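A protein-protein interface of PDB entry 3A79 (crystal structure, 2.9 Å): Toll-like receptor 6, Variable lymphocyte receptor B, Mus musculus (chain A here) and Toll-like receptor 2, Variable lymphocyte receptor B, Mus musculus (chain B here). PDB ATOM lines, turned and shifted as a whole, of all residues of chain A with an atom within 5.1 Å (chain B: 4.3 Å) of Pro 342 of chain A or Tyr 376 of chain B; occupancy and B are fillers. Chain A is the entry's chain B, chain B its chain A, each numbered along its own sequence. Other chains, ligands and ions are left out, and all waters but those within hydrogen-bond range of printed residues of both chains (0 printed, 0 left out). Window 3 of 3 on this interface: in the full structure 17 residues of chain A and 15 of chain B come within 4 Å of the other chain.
The backbone carbonyl oxygen of Pro 342 of chain A sits at hydrogen-bond distance from the side-chain hydroxyl of Tyr 376 of chain B (2.5 Å).
OG of Ser 380 of chain B is in hydrogen-bond range of O of Tyr 376 of chain B.
Phe 317 of chain A touches Glu 375 of chain B.
Asn 379 of chain B touches Phe 317 of chain A (ND2 to CD1, 3.5 Å).
Phe 349 of chain B touches Ile 344 of chain A (CE2 to CD1, 3.5 Å).
Ile 344 of chain A touches Tyr 376 of chain B.
Pro 342 of chain A touches just one residue of chain B: Tyr 376 (2.5 Å).
Printed residues of chain A within 4 Å of Tyr 376 of chain B: Pro 342 and Ile 344.
Of the printed residues of chain B, Ile 344 of chain A touches Phe 349 (3.5 Å) and Tyr 376 (3.8 Å).
Of the printed residues of chain A, Glu 375 of chain B touches Phe 317 (3.5 Å).
Of the printed residues of chain A, Asn 379 of chain B touches Phe 317.
Of the printed residues of chain B, Phe 317 of chain A touches Glu 375 and Asn 379.
Leu 350 of chain B touches none of the printed residues of chain A.
Leu 377 of chain B touches none of the printed residues of chain A.
The nearest printed residue of chain B that does not touch Pro 342 of chain A is Glu 375 of chain B (4.7 Å).
Hydrophobic or aromatic side chains of chain A within 4 Å of the printed part of chain B: Phe 317, Pro 342 and Ile 344.
Among the printed residues, no Asp or Glu carboxylate lies within 4 Å of a Lys or Arg side-chain nitrogen of the other chain.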
ATOM      1  N   VAL A 312      12.876 -15.703 -16.046  1.00  0.00           N
ATOM      2  CA  VAL A 312      13.992 -15.942 -16.934  1.00  0.00           C
ATOM      3  C   VAL A 312      13.801 -15.156 -18.206  1.00  0.00           C
ATOM      4  O   VAL A 312      12.846 -15.390 -18.942  1.00  0.00           O
ATOM      5  CB  VAL A 312      14.111 -17.425 -17.280  1.00  0.00           C
ATOM      6  CG1 VAL A 312      15.273 -17.643 -18.232  1.00  0.00           C
ATOM      7  CG2 VAL A 312      14.283 -18.244 -16.013  1.00  0.00           C
ATOM      8  N   LYS A 313      14.698 -14.206 -18.448  1.00  0.00           N
ATOM      9  CA  LYS A 313      14.701 -13.458 -19.698  1.00  0.00           C
ATOM     10  C   LYS A 313      15.716 -14.223 -20.610  1.00  0.00           C
ATOM     11  O   LYS A 313      16.766 -14.654 -20.138  1.00  0.00           O
ATOM     12  CB  LYS A 313      14.997 -11.923 -19.463  1.00  0.00           C
ATOM     13  CG  LYS A 313      14.489 -11.247 -18.053  1.00  0.00           C
ATOM     14  CD  LYS A 313      14.405  -9.626 -17.969  1.00  0.00           C
ATOM     15  CE  LYS A 313      13.889  -9.027 -16.559  1.00  0.00           C
ATOM     16  NZ  LYS A 313      13.476  -7.515 -16.303  1.00  0.00           N
ATOM     17  N   ASN A 314      15.384 -14.480 -21.877  1.00  0.00           N
ATOM     18  CA  ASN A 314      16.342 -15.135 -22.797  1.00  0.00           C
ATOM     19  C   ASN A 314      16.612 -14.354 -24.097  1.00  0.00           C
ATOM     20  O   ASN A 314      15.697 -14.061 -24.857  1.00  0.00           O
ATOM     21  CB  ASN A 314      15.921 -16.576 -23.112  1.00  0.00           C
ATOM     22  CG  ASN A 314      16.830 -17.253 -24.151  1.00  0.00           C
ATOM     23  OD1 ASN A 314      17.837 -16.696 -24.581  1.00  0.00           O
ATOM     24  ND2 ASN A 314      16.461 -18.464 -24.556  1.00  0.00           N
ATOM     25  N   PHE A 317      17.718 -16.513 -29.739  1.00  0.00           N
ATOM     26  CA  PHE A 317      16.457 -16.920 -30.383  1.00  0.00           C
ATOM     27  C   PHE A 317      16.563 -18.164 -31.224  1.00  0.00           C
ATOM     28  O   PHE A 317      15.627 -18.973 -31.258  1.00  0.00           O
ATOM     29  CB  PHE A 317      15.822 -15.781 -31.181  1.00  0.00           C
ATOM     30  CG  PHE A 317      15.347 -14.675 -30.316  1.00  0.00           C
ATOM     31  CD1 PHE A 317      16.075 -13.511 -30.199  1.00  0.00           C
ATOM     32  CD2 PHE A 317      14.213 -14.829 -29.552  1.00  0.00           C
ATOM     33  CE1 PHE A 317      15.656 -12.507 -29.377  1.00  0.00           C
ATOM     34  CE2 PHE A 317      13.791 -13.820 -28.724  1.00  0.00           C
ATOM     35  CZ  PHE A 317      14.516 -12.659 -28.632  1.00  0.00           C
ATOM     36  N   ASP A 340       7.971 -18.556 -14.779  1.00  0.00           N
ATOM     37  CA  ASP A 340       8.050 -17.208 -15.344  1.00  0.00           C
ATOM     38  C   ASP A 340       9.199 -17.054 -16.358  1.00  0.00           C
ATOM     39  O   ASP A 340      10.076 -16.206 -16.206  1.00  0.00           O
ATOM     40  CB  ASP A 340       8.176 -16.185 -14.219  1.00  0.00           C
ATOM     41  CG  ASP A 340       8.039 -14.753 -14.700  1.00  0.00           C
ATOM     42  OD1 ASP A 340       7.680 -14.521 -15.882  1.00  0.00           O
ATOM     43  OD2 ASP A 340       8.297 -13.855 -13.870  1.00  0.00           O
ATOM     44  N   THR A 341       9.167 -17.874 -17.402  1.00  0.00           N
ATOM     45  CA  THR A 341      10.199 -17.883 -18.418  1.00  0.00           C
ATOM     46  C   THR A 341       9.519 -17.936 -19.770  1.00  0.00           C
ATOM     47  O   THR A 341       8.321 -18.182 -19.844  1.00  0.00           O
ATOM     48  CB  THR A 341      11.011 -19.155 -18.305  1.00  0.00           C
ATOM     49  OG1 THR A 341      10.335 -20.190 -19.027  1.00  0.00           O
ATOM     50  CG2 THR A 341      11.148 -19.568 -16.847  1.00  0.00           C
ATOM     51  N   PRO A 342      10.284 -17.737 -20.854  1.00  0.00           N
ATOM     52  CA  PRO A 342       9.740 -17.875 -22.210  1.00  0.00           C
ATOM     53  C   PRO A 342       9.691 -19.325 -22.690  1.00  0.00           C
ATOM     54  O   PRO A 342       9.405 -19.542 -23.866  1.00  0.00           O
ATOM     55  CB  PRO A 342      10.754 -17.127 -23.079  1.00  0.00           C
ATOM     56  CG  PRO A 342      11.821 -16.618 -22.145  1.00  0.00           C
ATOM     57  CD  PRO A 342      11.703 -17.361 -20.872  1.00  0.00           C
ATOM     58  N   PHE A 343       9.972 -20.295 -21.821  1.00  0.00           N
ATOM     59  CA  PHE A 343      10.087 -21.684 -22.270  1.00  0.00           C
ATOM     60  C   PHE A 343       8.769 -22.217 -22.838  1.00  0.00           C
ATOM     61  O   PHE A 343       7.695 -21.902 -22.332  1.00  0.00           O
ATOM     62  CB  PHE A 343      10.619 -22.597 -21.156  1.00  0.00           C
ATOM     63  CG  PHE A 343      11.962 -22.185 -20.620  1.00  0.00           C
ATOM     64  CD1 PHE A 343      12.795 -21.355 -21.355  1.00  0.00           C
ATOM     65  CD2 PHE A 343      12.401 -22.642 -19.389  1.00  0.00           C
ATOM     66  CE1 PHE A 343      14.033 -20.970 -20.859  1.00  0.00           C
ATOM     67  CE2 PHE A 343      13.644 -22.261 -18.894  1.00  0.00           C
ATOM     68  CZ  PHE A 343      14.455 -21.421 -19.630  1.00  0.00           C
ATOM     69  N   ILE A 344       8.865 -23.027 -23.891  1.00  0.00           N
ATOM     70  CA  ILE A 344       7.693 -23.536 -24.599  1.00  0.00           C
ATOM     71  C   ILE A 344       7.441 -25.019 -24.330  1.00  0.00           C
ATOM     72  O   ILE A 344       6.461 -25.594 -24.822  1.00  0.00           O
ATOM     73  CB  ILE A 344       7.856 -23.361 -26.110  1.00  0.00           C
ATOM     74  CG1 ILE A 344       9.117 -24.073 -26.582  1.00  0.00           C
ATOM     75  CG2 ILE A 344       7.938 -21.901 -26.477  1.00  0.00           C
ATOM     76  CD1 ILE A 344       9.336 -23.981 -28.079  1.00  0.00           C
ATOM     77  N   ASN A 363       4.819 -20.320 -17.784  1.00  0.00           N
ATOM     78  CA  ASN A 363       5.682 -20.341 -18.945  1.00  0.00           C
ATOM     79  C   ASN A 363       4.795 -20.314 -20.167  1.00  0.00           C
ATOM     80  O   ASN A 363       3.741 -19.694 -20.155  1.00  0.00           O
ATOM     81  CB  ASN A 363       6.549 -21.597 -18.942  1.00  0.00           C
ATOM     82  CG  ASN A 363       7.390 -21.709 -17.701  1.00  0.00           C
ATOM     83  OD1 ASN A 363       7.338 -22.719 -17.002  1.00  0.00           O
ATOM     84  ND2 ASN A 363       8.163 -20.665 -17.405  1.00  0.00           N
ATOM     85  N   VAL A 364       5.213 -21.005 -21.216  1.00  0.00           N
ATOM     86  CA  VAL A 364       4.400 -21.139 -22.407  1.00  0.00           C
ATOM     87  C   VAL A 364       4.370 -22.612 -22.838  1.00  0.00           C
ATOM     88  O   VAL A 364       4.514 -22.925 -24.020  1.00  0.00           O
ATOM     89  CB  VAL A 364       4.909 -20.218 -23.538  1.00  0.00           C
ATOM     90  CG1 VAL A 364       3.797 -19.968 -24.569  1.00  0.00           C
ATOM     91  CG2 VAL A 364       5.406 -18.883 -22.954  1.00  0.00           C
ATOM     92  N   PHE B 349       5.549 -20.145 -32.069  1.00  0.00           N
ATOM     93  CA  PHE B 349       6.092 -19.449 -30.908  1.00  0.00           C
ATOM     94  C   PHE B 349       7.143 -18.429 -31.277  1.00  0.00           C
ATOM     95  O   PHE B 349       7.635 -17.720 -30.410  1.00  0.00           O
ATOM     96  CB  PHE B 349       6.679 -20.426 -29.898  1.00  0.00           C
ATOM     97  CG  PHE B 349       7.836 -21.217 -30.425  1.00  0.00           C
ATOM     98  CD1 PHE B 349       9.119 -20.679 -30.433  1.00  0.00           C
ATOM     99  CD2 PHE B 349       7.646 -22.504 -30.909  1.00  0.00           C
ATOM    100  CE1 PHE B 349      10.201 -21.409 -30.917  1.00  0.00           C
ATOM    101  CE2 PHE B 349       8.715 -23.242 -31.395  1.00  0.00           C
ATOM    102  CZ  PHE B 349      10.000 -22.693 -31.398  1.00  0.00           C
ATOM    103  N   LEU B 350       7.495 -18.360 -32.557  1.00  0.00           N
ATOM    104  CA  LEU B 350       8.426 -17.339 -33.026  1.00  0.00           C
ATOM    105  C   LEU B 350       8.512 -17.292 -34.537  1.00  0.00           C
ATOM    106  O   LEU B 350       8.719 -18.314 -35.167  1.00  0.00           O
ATOM    107  CB  LEU B 350       9.825 -17.595 -32.473  1.00  0.00           C
ATOM    108  CG  LEU B 350      10.890 -16.725 -33.138  1.00  0.00           C
ATOM    109  CD1 LEU B 350      10.924 -15.363 -32.493  1.00  0.00           C
ATOM    110  CD2 LEU B 350      12.247 -17.382 -33.076  1.00  0.00           C
ATOM    111  N   VAL B 373       4.551 -14.401 -27.358  1.00  0.00           N
ATOM    112  CA  VAL B 373       4.627 -13.561 -26.179  1.00  0.00           C
ATOM    113  C   VAL B 373       5.585 -12.408 -26.503  1.00  0.00           C
ATOM    114  O   VAL B 373       6.478 -12.559 -27.331  1.00  0.00           O
ATOM    115  CB  VAL B 373       5.092 -14.367 -24.946  1.00  0.00           C
ATOM    116  CG1 VAL B 373       3.985 -15.290 -24.494  1.00  0.00           C
ATOM    117  CG2 VAL B 373       6.347 -15.175 -25.264  1.00  0.00           C
ATOM    118  N   GLU B 374       5.389 -11.253 -25.881  1.00  0.00           N
ATOM    119  CA  GLU B 374       6.184 -10.089 -26.226  1.00  0.00           C
ATOM    120  C   GLU B 374       7.653 -10.447 -26.468  1.00  0.00           C
ATOM    121  O   GLU B 374       8.301  -9.871 -27.347  1.00  0.00           O
ATOM    122  CB  GLU B 374       6.066  -9.013 -25.147  1.00  0.00           C
ATOM    123  CG  GLU B 374       4.672  -8.463 -24.954  1.00  0.00           C
ATOM    124  CD  GLU B 374       3.834  -9.334 -24.052  1.00  0.00           C
ATOM    125  OE1 GLU B 374       4.330 -10.391 -23.609  1.00  0.00           O
ATOM    126  OE2 GLU B 374       2.678  -8.958 -23.783  1.00  0.00           O
ATOM    127  N   GLU B 375       8.168 -11.402 -25.695  1.00  0.00           N
ATOM    128  CA  GLU B 375       9.578 -11.796 -25.778  1.00  0.00           C
ATOM    129  C   GLU B 375       9.971 -12.302 -27.164  1.00  0.00           C
ATOM    130  O   GLU B 375      11.006 -11.924 -27.696  1.00  0.00           O
ATOM    131  CB  GLU B 375       9.932 -12.821 -24.694  1.00  0.00           C
ATOM    132  CG  GLU B 375       9.664 -12.333 -23.267  1.00  0.00           C
ATOM    133  CD  GLU B 375       8.193 -12.444 -22.873  1.00  0.00           C
ATOM    134  OE1 GLU B 375       7.707 -13.589 -22.763  1.00  0.00           O
ATOM    135  OE2 GLU B 375       7.528 -11.400 -22.664  1.00  0.00           O
ATOM    136  N   TYR B 376       9.135 -13.143 -27.751  1.00  0.00           N
ATOM    137  CA  TYR B 376       9.343 -13.566 -29.126  1.00  0.00           C
ATOM    138  C   TYR B 376       8.922 -12.497 -30.123  1.00  0.00           C
ATOM    139  O   TYR B 376       9.637 -12.210 -31.079  1.00  0.00           O
ATOM    140  CB  TYR B 376       8.574 -14.848 -29.390  1.00  0.00           C
ATOM    141  CG  TYR B 376       9.050 -15.967 -28.517  1.00  0.00           C
ATOM    142  CD1 TYR B 376       8.266 -16.439 -27.484  1.00  0.00           C
ATOM    143  CD2 TYR B 376      10.307 -16.535 -28.707  1.00  0.00           C
ATOM    144  CE1 TYR B 376       8.709 -17.463 -26.671  1.00  0.00           C
ATOM    145  CE2 TYR B 376      10.761 -17.556 -27.896  1.00  0.00           C
ATOM    146  CZ  TYR B 376       9.957 -18.015 -26.879  1.00  0.00           C
ATOM    147  OH  TYR B 376      10.378 -19.027 -26.059  1.00  0.00           O
ATOM    148  N   LEU B 377       7.752 -11.919 -29.900  1.00  0.00           N
ATOM    149  CA  LEU B 377       7.230 -10.884 -30.785  1.00  0.00           C
ATOM    150  C   LEU B 377       8.251  -9.775 -30.999  1.00  0.00           C
ATOM    151  O   LEU B 377       8.270  -9.141 -32.055  1.00  0.00           O
ATOM    152  CB  LEU B 377       5.942 -10.297 -30.213  1.00  0.00           C
ATOM    153  CG  LEU B 377       5.122  -9.398 -31.124  1.00  0.00           C
ATOM    154  CD1 LEU B 377       4.621 -10.214 -32.300  1.00  0.00           C
ATOM    155  CD2 LEU B 377       3.971  -8.775 -30.341  1.00  0.00           C
ATOM    156  N   LYS B 378       9.102  -9.545 -29.999  1.00  0.00           N
ATOM    157  CA  LYS B 378      10.111  -8.503 -30.111  1.00  0.00           C
ATOM    158  C   LYS B 378      11.149  -8.877 -31.151  1.00  0.00           C
ATOM    159  O   LYS B 378      11.736  -8.014 -31.789  1.00  0.00           O
ATOM    160  CB  LYS B 378      10.781  -8.210 -28.775  1.00  0.00           C
ATOM    161  CG  LYS B 378      11.659  -6.965 -28.812  1.00  0.00           C
ATOM    162  CD  LYS B 378      12.294  -6.686 -27.462  1.00  0.00           C
ATOM    163  CE  LYS B 378      12.603  -5.207 -27.281  1.00  0.00           C
ATOM    164  NZ  LYS B 378      12.948  -4.921 -25.857  1.00  0.00           N
ATOM    165  N   ASN B 379      11.376 -10.168 -31.334  1.00  0.00           N
ATOM    166  CA  ASN B 379      12.288 -10.588 -32.382  1.00  0.00           C
ATOM    167  C   ASN B 379      11.578 -10.681 -33.714  1.00  0.00           C
ATOM    168  O   ASN B 379      12.123 -10.297 -34.749  1.00  0.00           O
ATOM    169  CB  ASN B 379      12.942 -11.927 -32.069  1.00  0.00           C
ATOM    170  CG  ASN B 379      14.113 -12.211 -32.979  1.00  0.00           C
ATOM    171  OD1 ASN B 379      14.085 -13.146 -33.785  1.00  0.00           O
ATOM    172  ND2 ASN B 379      15.146 -11.383 -32.874  1.00  0.00           N
ATOM    173  N   SER B 380      10.357 -11.199 -33.683  1.00  0.00           N
ATOM    174  CA  SER B 380       9.612 -11.417 -34.908  1.00  0.00           C
ATOM    175  C   SER B 380       9.253 -10.104 -35.595  1.00  0.00           C
ATOM    176  O   SER B 380       9.118 -10.061 -36.814  1.00  0.00           O
ATOM    177  CB  SER B 380       8.386 -12.274 -34.636  1.00  0.00           C
ATOM    178  OG  SER B 380       8.794 -13.533 -34.135  1.00  0.00           O
